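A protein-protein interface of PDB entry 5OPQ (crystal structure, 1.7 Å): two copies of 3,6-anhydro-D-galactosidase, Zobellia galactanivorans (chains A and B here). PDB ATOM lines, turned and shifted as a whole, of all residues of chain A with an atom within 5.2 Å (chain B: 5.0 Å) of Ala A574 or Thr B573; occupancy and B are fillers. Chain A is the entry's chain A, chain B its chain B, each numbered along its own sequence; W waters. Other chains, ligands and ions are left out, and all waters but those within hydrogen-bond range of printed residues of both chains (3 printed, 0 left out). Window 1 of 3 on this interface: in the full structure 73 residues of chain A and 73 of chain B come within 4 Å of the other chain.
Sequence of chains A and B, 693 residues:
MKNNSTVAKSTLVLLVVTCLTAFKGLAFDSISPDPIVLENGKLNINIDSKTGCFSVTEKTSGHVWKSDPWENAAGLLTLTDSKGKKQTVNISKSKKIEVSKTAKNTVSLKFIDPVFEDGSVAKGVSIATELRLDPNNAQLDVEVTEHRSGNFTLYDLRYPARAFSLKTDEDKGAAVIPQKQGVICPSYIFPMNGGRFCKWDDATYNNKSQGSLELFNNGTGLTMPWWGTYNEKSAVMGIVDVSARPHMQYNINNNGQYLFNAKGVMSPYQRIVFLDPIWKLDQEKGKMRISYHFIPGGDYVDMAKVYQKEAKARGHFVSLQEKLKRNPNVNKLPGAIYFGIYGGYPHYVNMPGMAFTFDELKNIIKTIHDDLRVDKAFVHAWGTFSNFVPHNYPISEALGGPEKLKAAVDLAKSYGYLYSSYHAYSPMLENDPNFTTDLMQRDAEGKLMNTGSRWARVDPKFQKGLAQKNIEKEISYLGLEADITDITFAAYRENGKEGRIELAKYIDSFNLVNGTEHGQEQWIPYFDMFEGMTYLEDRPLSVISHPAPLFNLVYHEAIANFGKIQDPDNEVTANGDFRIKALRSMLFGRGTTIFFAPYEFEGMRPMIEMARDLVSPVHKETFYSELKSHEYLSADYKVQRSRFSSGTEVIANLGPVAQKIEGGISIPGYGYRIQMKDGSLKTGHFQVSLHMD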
ATOM      1  N   ARG A 196       6.095 -28.779 -16.948  1.00  0.00           N
ATOM      2  CA  ARG A 196       5.363 -29.986 -16.540  1.00  0.00           C
ATOM      3  C   ARG A 196       5.980 -30.541 -15.304  1.00  0.00           C
ATOM      4  O   ARG A 196       5.269 -31.078 -14.421  1.00  0.00           O
ATOM      5  CB  ARG A 196       5.406 -31.045 -17.661  1.00  0.00           C
ATOM      6  CG  ARG A 196       4.808 -30.596 -18.988  1.00  0.00           C
ATOM      7  CD  ARG A 196       3.286 -30.416 -18.856  1.00  0.00           C
ATOM      8  NE  ARG A 196       2.684 -30.043 -20.136  1.00  0.00           N
ATOM      9  CZ  ARG A 196       1.384 -29.839 -20.344  1.00  0.00           C
ATOM     10  NH1 ARG A 196       0.532 -30.008 -19.327  1.00  0.00           N
ATOM     11  NH2 ARG A 196       0.968 -29.471 -21.509  1.00  0.00           N
ATOM     12  N   LYS A 199       5.008 -28.768 -12.054  1.00  0.00           N
ATOM     13  CA  LYS A 199       3.623 -29.147 -11.682  1.00  0.00           C
ATOM     14  C   LYS A 199       3.544 -30.556 -11.164  1.00  0.00           C
ATOM     15  O   LYS A 199       2.821 -30.805 -10.179  1.00  0.00           O
ATOM     16  CB  LYS A 199       2.670 -28.936 -12.847  1.00  0.00           C
ATOM     17  CG  LYS A 199       2.423 -27.472 -13.190  1.00  0.00           C
ATOM     18  CD  LYS A 199       1.512 -27.270 -14.356  1.00  0.00           C
ATOM     19  CE  LYS A 199       2.077 -27.628 -15.685  1.00  0.00           C
ATOM     20  NZ  LYS A 199       1.087 -27.519 -16.810  1.00  0.00           N
ATOM     21  N   GLU A 537     -10.754 -32.486 -19.909  1.00  0.00           N
ATOM     22  CA  GLU A 537      -9.686 -31.534 -19.940  1.00  0.00           C
ATOM     23  C   GLU A 537      -9.051 -31.218 -18.579  1.00  0.00           C
ATOM     24  O   GLU A 537      -7.808 -31.189 -18.458  1.00  0.00           O
ATOM     25  CB  GLU A 537     -10.234 -30.249 -20.680  1.00  0.00           C
ATOM     26  CG  GLU A 537     -10.585 -30.426 -22.124  1.00  0.00           C
ATOM     27  CD  GLU A 537     -11.422 -29.281 -22.629  1.00  0.00           C
ATOM     28  OE1 GLU A 537     -10.906 -28.139 -22.677  1.00  0.00           O
ATOM     29  OE2 GLU A 537     -12.594 -29.483 -23.030  1.00  0.00           O
ATOM     30  N   ASP A 538      -9.867 -30.897 -17.651  1.00  0.00           N
ATOM     31  CA  ASP A 538      -9.496 -30.567 -16.256  1.00  0.00           C
ATOM     32  C   ASP A 538      -9.956 -31.788 -15.474  1.00  0.00           C
ATOM     33  O   ASP A 538     -11.122 -32.123 -15.486  1.00  0.00           O
ATOM     34  CB  ASP A 538     -10.345 -29.384 -15.735  1.00  0.00           C
ATOM     35  CG  ASP A 538     -10.032 -28.094 -16.435  1.00  0.00           C
ATOM     36  OD1 ASP A 538      -8.931 -27.994 -17.003  1.00  0.00           O
ATOM     37  OD2 ASP A 538     -10.880 -27.182 -16.390  1.00  0.00           O
ATOM     38  N   VAL A 572      -7.745 -26.409 -29.436  1.00  0.00           N
ATOM     39  CA  VAL A 572      -6.512 -26.531 -28.714  1.00  0.00           C
ATOM     40  C   VAL A 572      -6.835 -26.444 -27.236  1.00  0.00           C
ATOM     41  O   VAL A 572      -7.403 -25.433 -26.758  1.00  0.00           O
ATOM     42  CB  VAL A 572      -5.535 -25.396 -29.066  1.00  0.00           C
ATOM     43  CG1 VAL A 572      -4.304 -25.560 -28.291  1.00  0.00           C
ATOM     44  CG2 VAL A 572      -5.279 -25.454 -30.587  1.00  0.00           C
ATOM     45  N   THR A 573      -6.539 -27.510 -26.537  1.00  0.00           N
ATOM     46  CA  THR A 573      -6.928 -27.623 -25.114  1.00  0.00           C
ATOM     47  C   THR A 573      -5.854 -28.244 -24.279  1.00  0.00           C
ATOM     48  O   THR A 573      -4.725 -28.581 -24.783  1.00  0.00           O
ATOM     49  CB  THR A 573      -8.186 -28.499 -24.925  1.00  0.00           C
ATOM     50  OG1 THR A 573      -7.865 -29.826 -25.240  1.00  0.00           O
ATOM     51  CG2 THR A 573      -9.297 -28.135 -25.904  1.00  0.00           C
ATOM     52  N   ALA A 574      -6.186 -28.444 -23.000  1.00  0.00           N
ATOM     53  CA  ALA A 574      -5.261 -29.178 -22.098  1.00  0.00           C
ATOM     54  C   ALA A 574      -4.793 -30.486 -22.685  1.00  0.00           C
ATOM     55  O   ALA A 574      -3.729 -31.000 -22.313  1.00  0.00           O
ATOM     56  CB  ALA A 574      -5.906 -29.376 -20.732  1.00  0.00           C
ATOM     57  N   ASN A 575      -5.624 -31.099 -23.538  1.00  0.00           N
ATOM     58  CA  ASN A 575      -5.336 -32.451 -24.112  1.00  0.00           C
ATOM     59  C   ASN A 575      -4.612 -32.416 -25.426  1.00  0.00           C
ATOM     60  O   ASN A 575      -4.292 -33.433 -26.005  1.00  0.00           O
ATOM     61  CB  ASN A 575      -6.606 -33.263 -24.222  1.00  0.00           C
ATOM     62  CG  ASN A 575      -7.113 -33.643 -22.859  1.00  0.00           C
ATOM     63  OD1 ASN A 575      -6.316 -33.984 -21.994  1.00  0.00           O
ATOM     64  ND2 ASN A 575      -8.421 -33.597 -22.686  1.00  0.00           N
ATOM     65  N   GLY A 576      -4.311 -31.196 -25.854  1.00  0.00           N
ATOM     66  CA  GLY A 576      -3.405 -30.998 -27.033  1.00  0.00           C
ATOM     67  C   GLY A 576      -4.028 -30.174 -28.135  1.00  0.00           C
ATOM     68  O   GLY A 576      -5.200 -29.710 -28.048  1.00  0.00           O
ATOM     69  N   GLU B 537      -3.993 -22.532 -15.870  1.00  0.00           N
ATOM     70  CA  GLU B 537      -4.557 -23.417 -16.897  1.00  0.00           C
ATOM     71  C   GLU B 537      -6.004 -23.884 -16.581  1.00  0.00           C
ATOM     72  O   GLU B 537      -6.944 -23.726 -17.413  1.00  0.00           O
ATOM     73  CB  GLU B 537      -3.602 -24.605 -17.098  1.00  0.00           C
ATOM     74  CG  GLU B 537      -2.253 -24.199 -17.739  1.00  0.00           C
ATOM     75  CD  GLU B 537      -1.165 -25.282 -17.609  1.00  0.00           C
ATOM     76  OE1 GLU B 537      -1.441 -26.389 -18.136  1.00  0.00           O
ATOM     77  OE2 GLU B 537      -0.249 -25.106 -16.789  1.00  0.00           O
ATOM     78  N   ASP B 567       3.444 -22.780 -17.848  1.00  0.00           N
ATOM     79  CA  ASP B 567       2.632 -22.729 -19.030  1.00  0.00           C
ATOM     80  C   ASP B 567       3.306 -21.857 -20.051  1.00  0.00           C
ATOM     81  O   ASP B 567       2.762 -20.887 -20.527  1.00  0.00           O
ATOM     82  CB  ASP B 567       1.270 -22.087 -18.634  1.00  0.00           C
ATOM     83  CG  ASP B 567       0.275 -22.143 -19.711  1.00  0.00           C
ATOM     84  OD1 ASP B 567       0.380 -22.935 -20.656  1.00  0.00           O
ATOM     85  OD2 ASP B 567      -0.643 -21.293 -19.680  1.00  0.00           O
ATOM     86  N   GLU B 571       4.749 -24.895 -24.657  1.00  0.00           N
ATOM     87  CA  GLU B 571       3.877 -26.017 -24.206  1.00  0.00           C
ATOM     88  C   GLU B 571       2.463 -25.789 -24.718  1.00  0.00           C
ATOM     89  O   GLU B 571       2.005 -24.657 -24.786  1.00  0.00           O
ATOM     90  CB  GLU B 571       3.890 -26.062 -22.690  1.00  0.00           C
ATOM     91  CG  GLU B 571       5.119 -26.809 -22.118  1.00  0.00           C
ATOM     92  CD  GLU B 571       5.054 -28.296 -22.433  1.00  0.00           C
ATOM     93  OE1 GLU B 571       4.002 -28.932 -22.295  1.00  0.00           O
ATOM     94  OE2 GLU B 571       5.988 -28.860 -23.012  1.00  0.00           O
ATOM     95  N   VAL B 572       1.815 -26.889 -25.073  1.00  0.00           N
ATOM     96  CA  VAL B 572       0.436 -26.854 -25.526  1.00  0.00           C
ATOM     97  C   VAL B 572      -0.435 -27.121 -24.352  1.00  0.00           C
ATOM     98  O   VAL B 572      -0.379 -28.227 -23.763  1.00  0.00           O
ATOM     99  CB  VAL B 572       0.171 -27.893 -26.638  1.00  0.00           C
ATOM    100  CG1 VAL B 572      -1.260 -27.704 -27.139  1.00  0.00           C
ATOM    101  CG2 VAL B 572       1.140 -27.717 -27.818  1.00  0.00           C
ATOM    102  N   THR B 573      -1.232 -26.147 -23.980  1.00  0.00           N
ATOM    103  CA  THR B 573      -2.079 -26.254 -22.754  1.00  0.00           C
ATOM    104  C   THR B 573      -3.485 -25.708 -22.982  1.00  0.00           C
ATOM    105  O   THR B 573      -3.857 -25.238 -24.107  1.00  0.00           O
ATOM    106  CB  THR B 573      -1.461 -25.518 -21.581  1.00  0.00           C
ATOM    107  OG1 THR B 573      -1.594 -24.061 -21.809  1.00  0.00           O
ATOM    108  CG2 THR B 573      -0.025 -25.842 -21.333  1.00  0.00           C
ATOM    109  N   ALA B 574      -4.261 -25.669 -21.896  1.00  0.00           N
ATOM    110  CA  ALA B 574      -5.579 -25.105 -21.981  1.00  0.00           C
ATOM    111  C   ALA B 574      -5.513 -23.655 -22.439  1.00  0.00           C
ATOM    112  O   ALA B 574      -6.479 -23.135 -22.984  1.00  0.00           O
ATOM    113  CB  ALA B 574      -6.200 -25.147 -20.613  1.00  0.00           C
ATOM    114  N   ASN B 575      -4.385 -22.972 -22.205  1.00  0.00           N
ATOM    115  CA  ASN B 575      -4.231 -21.572 -22.649  1.00  0.00           C
ATOM    116  C   ASN B 575      -3.665 -21.341 -24.068  1.00  0.00           C
ATOM    117  O   ASN B 575      -3.512 -20.170 -24.543  1.00  0.00           O
ATOM    118  CB  ASN B 575      -3.403 -20.796 -21.609  1.00  0.00           C
ATOM    119  CG  ASN B 575      -4.153 -20.646 -20.319  1.00  0.00           C
ATOM    120  OD1 ASN B 575      -5.368 -20.408 -20.317  1.00  0.00           O
ATOM    121  ND2 ASN B 575      -3.450 -20.776 -19.235  1.00  0.00           N
ATOM    122  N   GLY B 576      -3.489 -22.419 -24.784  1.00  0.00           N
ATOM    123  CA  GLY B 576      -3.136 -22.401 -26.184  1.00  0.00           C
ATOM    124  C   GLY B 576      -1.843 -23.105 -26.542  1.00  0.00           C
ATOM    125  O   GLY B 576      -1.129 -23.645 -25.678  1.00  0.00           O
ATOM    126  N   ASP B 577      -1.569 -23.070 -27.869  1.00  0.00           N
ATOM    127  CA  ASP B 577      -0.331 -23.552 -28.455  1.00  0.00           C
ATOM    128  C   ASP B 577       0.516 -22.314 -28.752  1.00  0.00           C
ATOM    129  O   ASP B 577       0.209 -21.223 -28.251  1.00  0.00           O
ATOM    130  CB  ASP B 577      -0.652 -24.379 -29.696  1.00  0.00           C
ATOM    131  CG  ASP B 577      -1.404 -23.608 -30.741  1.00  0.00           C
ATOM    132  OD1 ASP B 577      -1.704 -22.391 -30.503  1.00  0.00           O
ATOM    133  OD2 ASP B 577      -1.754 -24.198 -31.804  1.00  0.00           O
ATOM    134  N   LYS B 581      -0.574 -18.314 -28.180  1.00  0.00           N
ATOM    135  CA  LYS B 581       0.187 -17.662 -27.149  1.00  0.00           C
ATOM    136  C   LYS B 581       0.991 -16.477 -27.765  1.00  0.00           C
ATOM    137  O   LYS B 581       1.060 -15.411 -27.147  1.00  0.00           O
ATOM    138  CB  LYS B 581       1.025 -18.549 -26.360  1.00  0.00           C
ATOM    139  CG  LYS B 581       0.157 -19.423 -25.420  1.00  0.00           C
ATOM    140  CD  LYS B 581       1.019 -20.541 -24.806  1.00  0.00           C
ATOM    141  CE  LYS B 581       0.273 -21.305 -23.670  1.00  0.00           C
ATOM    142  NZ  LYS B 581       1.099 -22.405 -23.177  1.00  0.00           N
HETATM  143  O   HOH W   1      -1.372 -30.663 -24.407  1.00  0.00           O
HETATM  144  O   HOH W   2      -6.446 -22.924 -26.116  1.00  0.00           O
HETATM  145  O   HOH W   3      -1.730 -28.566 -16.382  1.00  0.00           O
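NE of Arg A196 is in salt-bridge range of OE1 of Glu B571 (2.8 Å). The guanidinium group (NH2) of Arg A196 sits at hydrogen-bond distance from the backbone carbonyl oxygen (O) of Val B572. OE2 of Glu B537 lies within salt-bridge range of NZ of Lys A199 (2.8 Å).
OG1 of Thr A573 sits close to N of Asn A575, at 3.1 Å. The side-chain carboxylate (OD1) of Asp B567 lies within hydrogen-bond range of the side-chain hydroxyl (OG1) of Thr B573 (2.5 Å). The side-chain amino group of Lys B581 is in hydrogen-bond range of the backbone carbonyl oxygen of Glu B571, at 2.9 Å. N of Asn B575 sits close to OG1 of Thr B573. The side-chain amino group (NZ) of Lys B581 is in hydrogen-bond range of the side-chain hydroxyl (OG1) of Thr B573, 3.4 Å away.
Water W1 lies within hydrogen-bond range of O of Val B572 (2.7 Å), O of Ala A574 (3.2 Å) and N of Gly A576 (3.3 Å). Water W2 lies within hydrogen-bond range of O of Val A572 (2.8 Å), O of Ala B574 (3.1 Å) and N of Gly B576 (3.3 Å). Water W3 lies within hydrogen-bond range of OE1 of Glu B537 (2.8 Å) and NZ of Lys A199 (3.0 Å).
NH2 of Arg A196 touches CG2 of Thr B573 (3.8 Å). CG1 of Val B572 touches CG1 of Val A572 (3.9 Å). CG1 of Val A572 touches C of Gly B576, 3.9 Å away. Asp B577 touches Val A572 (N to CG1, 3.7 Å). Thr A573 touches Thr B573. C of Thr A573 touches N of Ala B574, at 3.9 Å. Thr B573 touches Ala A574. Ala A574 touches Ala B574 (N to CA, 3.5 Å). Val B572 touches Gly A576.
Of chain A, only Arg A196, Thr A573 and Ala A574 come within 4 Å of Thr B573. Of the printed residues of chain B, Lys A199 touches Glu B537. Of the printed residues of chain A, Ala B574 touches Thr A573 and Ala A574. Of the printed residues of chain A, Glu B537 touches Lys A199 (2.8 Å). Printed residues of chain B within 4 Å of Gly A576: Val B572. The nearest printed residue of chain A that does not touch Glu B571 is Lys A199 (6.4 Å).
Of the 10 printed residues of chain B, 7 touch a printed residue of chain A. Hydrophobic or aromatic side chains of chain B within 4 Å of the printed part of chain A: Val B572. Of the 9 printed residues of chain A, 6 touch a printed residue of chain B. Printed residues of chain A that touch a printed residue of chain B: Arg A196, Lys A199, Val A572, Thr A573, Ala A574 and Gly A576. Hydrophobic or aromatic side chains of chain A that line the printed part of chain B: Val A572. Among the printed residues, 12 pairs touch across the chains.
Val A572 touches its own counterpart, Val B572. Val A572 touches Gly B576, and with the chains exchanged Gly A576 touches Val B572. Thr A573 touches its own counterpart, Thr B573. Ala B574 touches its own counterpart, Ala A574. Positions printed for both chains: 537, 572, 573, 574, 575 and 576.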
